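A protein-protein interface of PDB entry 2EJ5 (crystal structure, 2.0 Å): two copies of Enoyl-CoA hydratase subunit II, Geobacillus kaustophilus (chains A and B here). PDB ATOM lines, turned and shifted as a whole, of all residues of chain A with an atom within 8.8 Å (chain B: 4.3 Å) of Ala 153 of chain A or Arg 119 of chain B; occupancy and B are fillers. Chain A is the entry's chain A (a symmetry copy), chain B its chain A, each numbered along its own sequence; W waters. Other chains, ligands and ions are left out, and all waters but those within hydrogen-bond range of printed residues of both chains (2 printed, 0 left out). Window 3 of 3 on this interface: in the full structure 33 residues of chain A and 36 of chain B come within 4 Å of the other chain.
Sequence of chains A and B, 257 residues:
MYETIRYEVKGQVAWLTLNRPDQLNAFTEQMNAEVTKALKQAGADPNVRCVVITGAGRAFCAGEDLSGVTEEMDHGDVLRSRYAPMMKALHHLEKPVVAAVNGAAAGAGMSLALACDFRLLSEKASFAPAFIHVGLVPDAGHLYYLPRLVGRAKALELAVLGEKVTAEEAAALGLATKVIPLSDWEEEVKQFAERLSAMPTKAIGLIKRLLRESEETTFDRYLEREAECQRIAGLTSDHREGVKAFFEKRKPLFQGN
The backbone NH of Ala 99 of chain B lies within hydrogen-bond range of the backbone carbonyl oxygen of Phe 118 of chain B (2.8 Å). NE of Arg 119 of chain B sits at hydrogen-bond distance from O of Leu 175 of chain B, 3.0 Å away. The backbone carbonyl oxygen (O) of Ala 113 of chain B is in hydrogen-bond range of the guanidinium group (NH1) of Arg 119 of chain B (2.9 Å). NZ of Lys 154 of chain A lies within salt-bridge range of OE2 of Glu 157 of chain A, at 3.5 Å. The guanidinium group (NH1) of Arg 119 of chain B lies within hydrogen-bond range of the backbone carbonyl oxygen (O) of Cys 116 of chain B, at 2.9 Å. The backbone carbonyl oxygen (O) of Leu 114 of chain B lies within hydrogen-bond range of the guanidinium group (NH1) of Arg 119 of chain B (3.3 Å).
Ala 153 of chain A touches Arg 119 of chain B. Leu 149 of chain B touches Ala 153 of chain A (CD2 to N, 3.5 Å). Phe 118 of chain B touches Leu 156 of chain A (CZ to CD2, 3.3 Å). Glu 157 of chain A touches Phe 118 of chain B (CA to CE1, 3.9 Å). Thr 177 of chain B touches Glu 157 of chain A. Val 160 of chain A touches Phe 118 of chain B (CG1 to CZ, 3.8 Å).
Ala 153 of chain A touches two residues of chain B. Arg 119 of chain B touches one residue of chain A. Of the printed residues of chain A, Thr 177 of chain B touches Glu 157. Printed residues of chain B within 4 Å of Val 160 of chain A: Phe 118. Printed residues of chain A within 4 Å of Leu 149 of chain B: Ala 153. Of the printed residues of chain B, Glu 157 of chain A touches Phe 118 (3.9 Å) and Thr 177 (3.9 Å). Printed residues of chain A within 4 Å of Phe 118 of chain B: Leu 156, Glu 157 and Val 160. Lys 178 of chain B touches none of the printed residues of chain A. Leu 173 of chain A touches none of the printed residues of chain B. The nearest residue of chain A that does not touch Arg 119 of chain B is Arg 152 of chain A (6.4 Å).
Of the 14 printed residues of chain B, 4 touch a printed residue of chain A. Hydrophobic or aromatic side chains of chain B within 4 Å of the printed part of chain A: Phe 118 and Leu 149. Of the 15 printed residues of chain A, 4 touch a printed residue of chain B. Printed residues of chain A that touch a printed residue of chain B: Ala 153, Leu 156, Glu 157 and Val 160. Among the printed residues, no Asp or Glu carboxylate lies within 4 Å of a Lys or Arg side-chain nitrogen of the other chain.
No position is printed for both chains.
Water W2 bridges the side-chain hydroxyl (OG1) of Thr 177 of chain B (2.5 Å) and the side-chain carboxylate (OE1) of Glu 157 of chain A (3.0 Å). Water W1 bridges OE1 of Glu 157 of chain A (2.7 Å) and O of Thr 177 of chain B (3.0 Å).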
ATOM      1  N   LEU A 146     -33.022  22.475 -20.153  1.00  0.00           N
ATOM      2  CA  LEU A 146     -31.628  22.724 -20.532  1.00  0.00           C
ATOM      3  C   LEU A 146     -30.918  21.431 -20.960  1.00  0.00           C
ATOM      4  O   LEU A 146     -30.285  21.432 -21.976  1.00  0.00           O
ATOM      5  CB  LEU A 146     -30.861  23.440 -19.415  1.00  0.00           C
ATOM      6  CG  LEU A 146     -29.466  23.938 -19.766  1.00  0.00           C
ATOM      7  CD1 LEU A 146     -29.487  24.847 -21.089  1.00  0.00           C
ATOM      8  CD2 LEU A 146     -28.838  24.635 -18.521  1.00  0.00           C
ATOM      9  N   PRO A 147     -30.995  20.343 -20.169  1.00  0.00           N
ATOM     10  CA  PRO A 147     -30.293  19.155 -20.677  1.00  0.00           C
ATOM     11  C   PRO A 147     -30.917  18.604 -21.962  1.00  0.00           C
ATOM     12  O   PRO A 147     -30.207  17.925 -22.724  1.00  0.00           O
ATOM     13  CB  PRO A 147     -30.450  18.121 -19.564  1.00  0.00           C
ATOM     14  CG  PRO A 147     -30.983  18.858 -18.386  1.00  0.00           C
ATOM     15  CD  PRO A 147     -31.655  20.092 -18.884  1.00  0.00           C
ATOM     16  N   VAL A 150     -28.886  20.891 -24.442  1.00  0.00           N
ATOM     17  CA  VAL A 150     -27.420  20.871 -24.484  1.00  0.00           C
ATOM     18  C   VAL A 150     -26.765  19.599 -23.909  1.00  0.00           C
ATOM     19  O   VAL A 150     -25.549  19.505 -23.929  1.00  0.00           O
ATOM     20  CB  VAL A 150     -26.797  22.149 -23.821  1.00  0.00           C
ATOM     21  CG1 VAL A 150     -27.240  23.440 -24.552  1.00  0.00           C
ATOM     22  CG2 VAL A 150     -27.202  22.242 -22.398  1.00  0.00           C
ATOM     23  N   GLY A 151     -27.547  18.642 -23.403  1.00  0.00           N
ATOM     24  CA  GLY A 151     -27.011  17.397 -22.795  1.00  0.00           C
ATOM     25  C   GLY A 151     -26.663  17.604 -21.333  1.00  0.00           C
ATOM     26  O   GLY A 151     -26.625  18.762 -20.870  1.00  0.00           O
ATOM     27  N   ARG A 152     -26.386  16.524 -20.597  1.00  0.00           N
ATOM     28  CA  ARG A 152     -26.272  16.663 -19.132  1.00  0.00           C
ATOM     29  C   ARG A 152     -25.085  17.491 -18.715  1.00  0.00           C
ATOM     30  O   ARG A 152     -25.177  18.259 -17.738  1.00  0.00           O
ATOM     31  CB  ARG A 152     -26.205  15.282 -18.440  1.00  0.00           C
ATOM     32  CG  ARG A 152     -25.928  15.343 -16.886  1.00  0.00           C
ATOM     33  CD  ARG A 152     -26.046  13.916 -16.278  1.00  0.00           C
ATOM     34  NE  ARG A 152     -26.622  13.786 -14.925  1.00  0.00           N
ATOM     35  CZ  ARG A 152     -27.913  13.890 -14.606  1.00  0.00           C
ATOM     36  NH1 ARG A 152     -28.807  14.232 -15.528  1.00  0.00           N
ATOM     37  NH2 ARG A 152     -28.328  13.680 -13.360  1.00  0.00           N
ATOM     38  N   ALA A 153     -23.949  17.264 -19.377  1.00  0.00           N
ATOM     39  CA  ALA A 153     -22.673  17.854 -18.912  1.00  0.00           C
ATOM     40  C   ALA A 153     -22.750  19.384 -19.034  1.00  0.00           C
ATOM     41  O   ALA A 153     -22.440  20.123 -18.083  1.00  0.00           O
ATOM     42  CB  ALA A 153     -21.482  17.329 -19.696  1.00  0.00           C
ATOM     43  N   LYS A 154     -23.159  19.867 -20.206  1.00  0.00           N
ATOM     44  CA  LYS A 154     -23.206  21.323 -20.391  1.00  0.00           C
ATOM     45  C   LYS A 154     -24.273  21.942 -19.507  1.00  0.00           C
ATOM     46  O   LYS A 154     -24.101  23.074 -19.042  1.00  0.00           O
ATOM     47  CB  LYS A 154     -23.395  21.718 -21.853  1.00  0.00           C
ATOM     48  CG  LYS A 154     -23.044  23.192 -22.078  1.00  0.00           C
ATOM     49  CD  LYS A 154     -21.502  23.365 -22.056  1.00  0.00           C
ATOM     50  CE  LYS A 154     -21.113  24.755 -21.619  1.00  0.00           C
ATOM     51  NZ  LYS A 154     -19.667  25.038 -21.999  1.00  0.00           N
ATOM     52  N   ALA A 155     -25.386  21.232 -19.275  1.00  0.00           N
ATOM     53  CA  ALA A 155     -26.415  21.794 -18.415  1.00  0.00           C
ATOM     54  C   ALA A 155     -25.887  21.963 -16.989  1.00  0.00           C
ATOM     55  O   ALA A 155     -26.169  22.971 -16.356  1.00  0.00           O
ATOM     56  CB  ALA A 155     -27.710  20.919 -18.402  1.00  0.00           C
ATOM     57  N   LEU A 156     -25.162  20.956 -16.497  1.00  0.00           N
ATOM     58  CA  LEU A 156     -24.568  21.013 -15.147  1.00  0.00           C
ATOM     59  C   LEU A 156     -23.510  22.152 -15.059  1.00  0.00           C
ATOM     60  O   LEU A 156     -23.485  22.910 -14.091  1.00  0.00           O
ATOM     61  CB  LEU A 156     -24.010  19.639 -14.759  1.00  0.00           C
ATOM     62  CG  LEU A 156     -23.592  19.528 -13.287  1.00  0.00           C
ATOM     63  CD1 LEU A 156     -23.821  18.133 -12.729  1.00  0.00           C
ATOM     64  CD2 LEU A 156     -22.148  19.963 -13.184  1.00  0.00           C
ATOM     65  N   GLU A 157     -22.697  22.294 -16.084  1.00  0.00           N
ATOM     66  CA  GLU A 157     -21.671  23.314 -16.127  1.00  0.00           C
ATOM     67  C   GLU A 157     -22.278  24.719 -16.062  1.00  0.00           C
ATOM     68  O   GLU A 157     -21.874  25.547 -15.235  1.00  0.00           O
ATOM     69  CB  GLU A 157     -20.765  23.138 -17.350  1.00  0.00           C
ATOM     70  CG  GLU A 157     -19.635  24.175 -17.352  1.00  0.00           C
ATOM     71  CD  GLU A 157     -18.689  24.058 -18.548  1.00  0.00           C
ATOM     72  OE1 GLU A 157     -18.590  22.962 -19.152  1.00  0.00           O
ATOM     73  OE2 GLU A 157     -18.017  25.098 -18.857  1.00  0.00           O
ATOM     74  N   LEU A 158     -23.323  24.932 -16.847  1.00  0.00           N
ATOM     75  CA  LEU A 158     -24.077  26.166 -16.822  1.00  0.00           C
ATOM     76  C   LEU A 158     -24.712  26.426 -15.477  1.00  0.00           C
ATOM     77  O   LEU A 158     -24.504  27.495 -14.923  1.00  0.00           O
ATOM     78  CB  LEU A 158     -25.139  26.147 -17.913  1.00  0.00           C
ATOM     79  CG  LEU A 158     -24.545  26.320 -19.327  1.00  0.00           C
ATOM     80  CD1 LEU A 158     -25.708  26.255 -20.283  1.00  0.00           C
ATOM     81  CD2 LEU A 158     -23.835  27.646 -19.481  1.00  0.00           C
ATOM     82  N   ALA A 159     -25.458  25.447 -14.943  1.00  0.00           N
ATOM     83  CA  ALA A 159     -26.097  25.579 -13.642  1.00  0.00           C
ATOM     84  C   ALA A 159     -25.120  25.749 -12.492  1.00  0.00           C
ATOM     85  O   ALA A 159     -25.448  26.431 -11.522  1.00  0.00           O
ATOM     86  CB  ALA A 159     -27.015  24.367 -13.339  1.00  0.00           C
ATOM     87  N   VAL A 160     -23.960  25.097 -12.560  1.00  0.00           N
ATOM     88  CA  VAL A 160     -23.085  25.013 -11.391  1.00  0.00           C
ATOM     89  C   VAL A 160     -22.075  26.128 -11.399  1.00  0.00           C
ATOM     90  O   VAL A 160     -21.884  26.811 -10.381  1.00  0.00           O
ATOM     91  CB  VAL A 160     -22.416  23.593 -11.207  1.00  0.00           C
ATOM     92  CG1 VAL A 160     -21.246  23.606 -10.188  1.00  0.00           C
ATOM     93  CG2 VAL A 160     -23.464  22.572 -10.825  1.00  0.00           C
ATOM     94  N   LEU A 161     -21.435  26.337 -12.538  1.00  0.00           N
ATOM     95  CA  LEU A 161     -20.416  27.378 -12.621  1.00  0.00           C
ATOM     96  C   LEU A 161     -21.050  28.744 -12.809  1.00  0.00           C
ATOM     97  O   LEU A 161     -20.470  29.763 -12.416  1.00  0.00           O
ATOM     98  CB  LEU A 161     -19.418  27.037 -13.715  1.00  0.00           C
ATOM     99  CG  LEU A 161     -18.625  25.756 -13.392  1.00  0.00           C
ATOM    100  CD1 LEU A 161     -17.704  25.389 -14.555  1.00  0.00           C
ATOM    101  CD2 LEU A 161     -17.833  25.847 -12.049  1.00  0.00           C
ATOM    102  N   LEU A 173     -23.409  26.755 -28.488  1.00  0.00           N
ATOM    103  CA  LEU A 173     -23.930  25.737 -27.555  1.00  0.00           C
ATOM    104  C   LEU A 173     -25.216  25.067 -28.056  1.00  0.00           C
ATOM    105  O   LEU A 173     -25.635  24.047 -27.533  1.00  0.00           O
ATOM    106  CB  LEU A 173     -24.178  26.349 -26.176  1.00  0.00           C
ATOM    107  CG  LEU A 173     -22.986  26.748 -25.316  1.00  0.00           C
ATOM    108  CD1 LEU A 173     -23.476  27.536 -24.077  1.00  0.00           C
ATOM    109  CD2 LEU A 173     -22.188  25.478 -24.940  1.00  0.00           C
ATOM    110  N   ALA B  99     -13.973  14.289 -12.396  1.00  0.00           N
ATOM    111  CA  ALA B  99     -13.053  13.255 -12.911  1.00  0.00           C
ATOM    112  C   ALA B  99     -11.846  13.984 -13.495  1.00  0.00           C
ATOM    113  O   ALA B  99     -11.978  14.691 -14.486  1.00  0.00           O
ATOM    114  CB  ALA B  99     -13.720  12.418 -13.966  1.00  0.00           C
ATOM    115  N   ALA B 113     -15.610   7.835 -15.500  1.00  0.00           N
ATOM    116  CA  ALA B 113     -15.409   9.233 -15.904  1.00  0.00           C
ATOM    117  C   ALA B 113     -16.723   9.890 -16.407  1.00  0.00           C
ATOM    118  O   ALA B 113     -17.038  11.032 -16.066  1.00  0.00           O
ATOM    119  CB  ALA B 113     -14.297   9.343 -16.943  1.00  0.00           C
ATOM    120  N   LEU B 114     -17.511   9.137 -17.183  1.00  0.00           N
ATOM    121  CA  LEU B 114     -18.777   9.646 -17.713  1.00  0.00           C
ATOM    122  C   LEU B 114     -19.789   9.919 -16.604  1.00  0.00           C
ATOM    123  O   LEU B 114     -20.682  10.772 -16.767  1.00  0.00           O
ATOM    124  CB  LEU B 114     -19.363   8.616 -18.692  1.00  0.00           C
ATOM    125  CG  LEU B 114     -18.548   8.195 -19.905  1.00  0.00           C
ATOM    126  CD1 LEU B 114     -19.347   7.177 -20.764  1.00  0.00           C
ATOM    127  CD2 LEU B 114     -18.138   9.432 -20.754  1.00  0.00           C
ATOM    128  N   CYS B 116     -19.133  11.156 -13.651  1.00  0.00           N
ATOM    129  CA  CYS B 116     -18.769  12.349 -12.877  1.00  0.00           C
ATOM    130  C   CYS B 116     -19.400  13.597 -13.466  1.00  0.00           C
ATOM    131  O   CYS B 116     -19.860  13.572 -14.586  1.00  0.00           O
ATOM    132  CB  CYS B 116     -17.246  12.492 -12.800  1.00  0.00           C
ATOM    133  SG  CYS B 116     -16.514  11.104 -11.823  1.00  0.00           S
ATOM    134  N   PHE B 118     -17.933  16.747 -13.929  1.00  0.00           N
ATOM    135  CA  PHE B 118     -16.989  17.437 -14.808  1.00  0.00           C
ATOM    136  C   PHE B 118     -15.870  16.471 -15.140  1.00  0.00           C
ATOM    137  O   PHE B 118     -15.539  15.600 -14.296  1.00  0.00           O
ATOM    138  CB  PHE B 118     -16.384  18.656 -14.089  1.00  0.00           C
ATOM    139  CG  PHE B 118     -17.406  19.646 -13.581  1.00  0.00           C
ATOM    140  CD1 PHE B 118     -17.922  20.640 -14.435  1.00  0.00           C
ATOM    141  CD2 PHE B 118     -17.837  19.606 -12.261  1.00  0.00           C
ATOM    142  CE1 PHE B 118     -18.851  21.573 -13.996  1.00  0.00           C
ATOM    143  CE2 PHE B 118     -18.767  20.542 -11.800  1.00  0.00           C
ATOM    144  CZ  PHE B 118     -19.276  21.540 -12.671  1.00  0.00           C
ATOM    145  N   ARG B 119     -15.293  16.602 -16.341  1.00  0.00           N
ATOM    146  CA  ARG B 119     -14.182  15.749 -16.798  1.00  0.00           C
ATOM    147  C   ARG B 119     -13.063  16.677 -17.299  1.00  0.00           C
ATOM    148  O   ARG B 119     -13.245  17.384 -18.300  1.00  0.00           O
ATOM    149  CB  ARG B 119     -14.607  14.815 -17.960  1.00  0.00           C
ATOM    150  CG  ARG B 119     -15.417  13.530 -17.533  1.00  0.00           C
ATOM    151  CD  ARG B 119     -16.214  12.893 -18.705  1.00  0.00           C
ATOM    152  NE  ARG B 119     -17.286  13.826 -19.006  1.00  0.00           N
ATOM    153  CZ  ARG B 119     -18.358  13.982 -18.235  1.00  0.00           C
ATOM    154  NH1 ARG B 119     -18.518  13.220 -17.165  1.00  0.00           N
ATOM    155  NH2 ARG B 119     -19.264  14.903 -18.516  1.00  0.00           N
ATOM    156  N   LEU B 120     -11.957  16.727 -16.556  1.00  0.00           N
ATOM    157  CA  LEU B 120     -10.805  17.524 -16.942  1.00  0.00           C
ATOM    158  C   LEU B 120      -9.851  16.516 -17.532  1.00  0.00           C
ATOM    159  O   LEU B 120      -9.405  15.617 -16.830  1.00  0.00           O
ATOM    160  CB  LEU B 120     -10.156  18.196 -15.709  1.00  0.00           C
ATOM    161  CG  LEU B 120     -11.027  19.063 -14.806  1.00  0.00           C
ATOM    162  CD1 LEU B 120     -10.213  19.612 -13.597  1.00  0.00           C
ATOM    163  CD2 LEU B 120     -11.653  20.245 -15.621  1.00  0.00           C
ATOM    164  N   LEU B 121      -9.543  16.663 -18.806  1.00  0.00           N
ATOM    165  CA  LEU B 121      -8.679  15.703 -19.462  1.00  0.00           C
ATOM    166  C   LEU B 121      -7.287  16.324 -19.610  1.00  0.00           C
ATOM    167  O   LEU B 121      -7.149  17.428 -20.115  1.00  0.00           O
ATOM    168  CB  LEU B 121      -9.231  15.336 -20.824  1.00  0.00           C
ATOM    169  CG  LEU B 121     -10.220  14.160 -20.950  1.00  0.00           C
ATOM    170  CD1 LEU B 121     -11.358  14.107 -19.946  1.00  0.00           C
ATOM    171  CD2 LEU B 121     -10.757  14.191 -22.376  1.00  0.00           C
ATOM    172  N   PHE B 127     -10.104   8.171 -24.165  1.00  0.00           N
ATOM    173  CA  PHE B 127     -11.217   7.359 -23.742  1.00  0.00           C
ATOM    174  C   PHE B 127     -11.251   6.178 -24.685  1.00  0.00           C
ATOM    175  O   PHE B 127     -11.224   6.348 -25.905  1.00  0.00           O
ATOM    176  CB  PHE B 127     -12.547   8.148 -23.790  1.00  0.00           C
ATOM    177  CG  PHE B 127     -12.754   9.110 -22.651  1.00  0.00           C
ATOM    178  CD1 PHE B 127     -12.572   8.714 -21.323  1.00  0.00           C
ATOM    179  CD2 PHE B 127     -13.212  10.410 -22.910  1.00  0.00           C
ATOM    180  CE1 PHE B 127     -12.816   9.606 -20.278  1.00  0.00           C
ATOM    181  CE2 PHE B 127     -13.452  11.315 -21.899  1.00  0.00           C
ATOM    182  CZ  PHE B 127     -13.286  10.921 -20.563  1.00  0.00           C
ATOM    183  N   LEU B 149     -25.090  12.398 -22.902  1.00  0.00           N
ATOM    184  CA  LEU B 149     -24.030  13.364 -23.155  1.00  0.00           C
ATOM    185  C   LEU B 149     -23.831  13.620 -24.639  1.00  0.00           C
ATOM    186  O   LEU B 149     -23.581  14.773 -25.040  1.00  0.00           O
ATOM    187  CB  LEU B 149     -22.693  12.906 -22.588  1.00  0.00           C
ATOM    188  CG  LEU B 149     -22.603  12.746 -21.081  1.00  0.00           C
ATOM    189  CD1 LEU B 149     -21.311  12.031 -20.665  1.00  0.00           C
ATOM    190  CD2 LEU B 149     -22.753  14.103 -20.426  1.00  0.00           C
ATOM    191  N   LEU B 175     -17.367  15.464 -24.441  1.00  0.00           N
ATOM    192  CA  LEU B 175     -16.964  14.600 -23.320  1.00  0.00           C
ATOM    193  C   LEU B 175     -15.906  15.172 -22.357  1.00  0.00           C
ATOM    194  O   LEU B 175     -15.593  14.544 -21.324  1.00  0.00           O
ATOM    195  CB  LEU B 175     -16.482  13.253 -23.867  1.00  0.00           C
ATOM    196  CG  LEU B 175     -17.544  12.410 -24.561  1.00  0.00           C
ATOM    197  CD1 LEU B 175     -16.902  11.103 -25.054  1.00  0.00           C
ATOM    198  CD2 LEU B 175     -18.657  12.111 -23.590  1.00  0.00           C
ATOM    199  N   ALA B 176     -15.354  16.333 -22.692  1.00  0.00           N
ATOM    200  CA  ALA B 176     -14.421  17.034 -21.794  1.00  0.00           C
ATOM    201  C   ALA B 176     -14.899  18.444 -21.391  1.00  0.00           C
ATOM    202  O   ALA B 176     -15.241  19.274 -22.229  1.00  0.00           O
ATOM    203  CB  ALA B 176     -13.007  17.117 -22.442  1.00  0.00           C
ATOM    204  N   THR B 177     -14.908  18.713 -20.092  1.00  0.00           N
ATOM    205  CA  THR B 177     -15.039  20.068 -19.583  1.00  0.00           C
ATOM    206  C   THR B 177     -13.883  20.963 -20.063  1.00  0.00           C
ATOM    207  O   THR B 177     -14.108  22.116 -20.463  1.00  0.00           O
ATOM    208  CB  THR B 177     -15.051  20.069 -18.080  1.00  0.00           C
ATOM    209  OG1 THR B 177     -16.047  19.136 -17.654  1.00  0.00           O
ATOM    210  CG2 THR B 177     -15.362  21.473 -17.562  1.00  0.00           C
ATOM    211  N   LYS B 178     -12.652  20.444 -19.991  1.00  0.00           N
ATOM    212  CA  LYS B 178     -11.526  21.085 -20.666  1.00  0.00           C
ATOM    213  C   LYS B 178     -10.366  20.120 -20.831  1.00  0.00           C
ATOM    214  O   LYS B 178     -10.337  19.073 -20.193  1.00  0.00           O
ATOM    215  CB  LYS B 178     -11.077  22.359 -19.936  1.00  0.00           C
ATOM    216  CG  LYS B 178     -10.840  22.269 -18.459  1.00  0.00           C
ATOM    217  CD  LYS B 178     -10.588  23.691 -17.926  1.00  0.00           C
ATOM    218  CE  LYS B 178     -10.521  23.724 -16.413  1.00  0.00           C
ATOM    219  NZ  LYS B 178      -9.933  24.998 -15.896  1.00  0.00           N
HETATM  220  O   HOH W   1     -16.770  23.212 -21.177  1.00  0.00           O
HETATM  221  O   HOH W   2     -18.240  20.076 -18.330  1.00  0.00           O
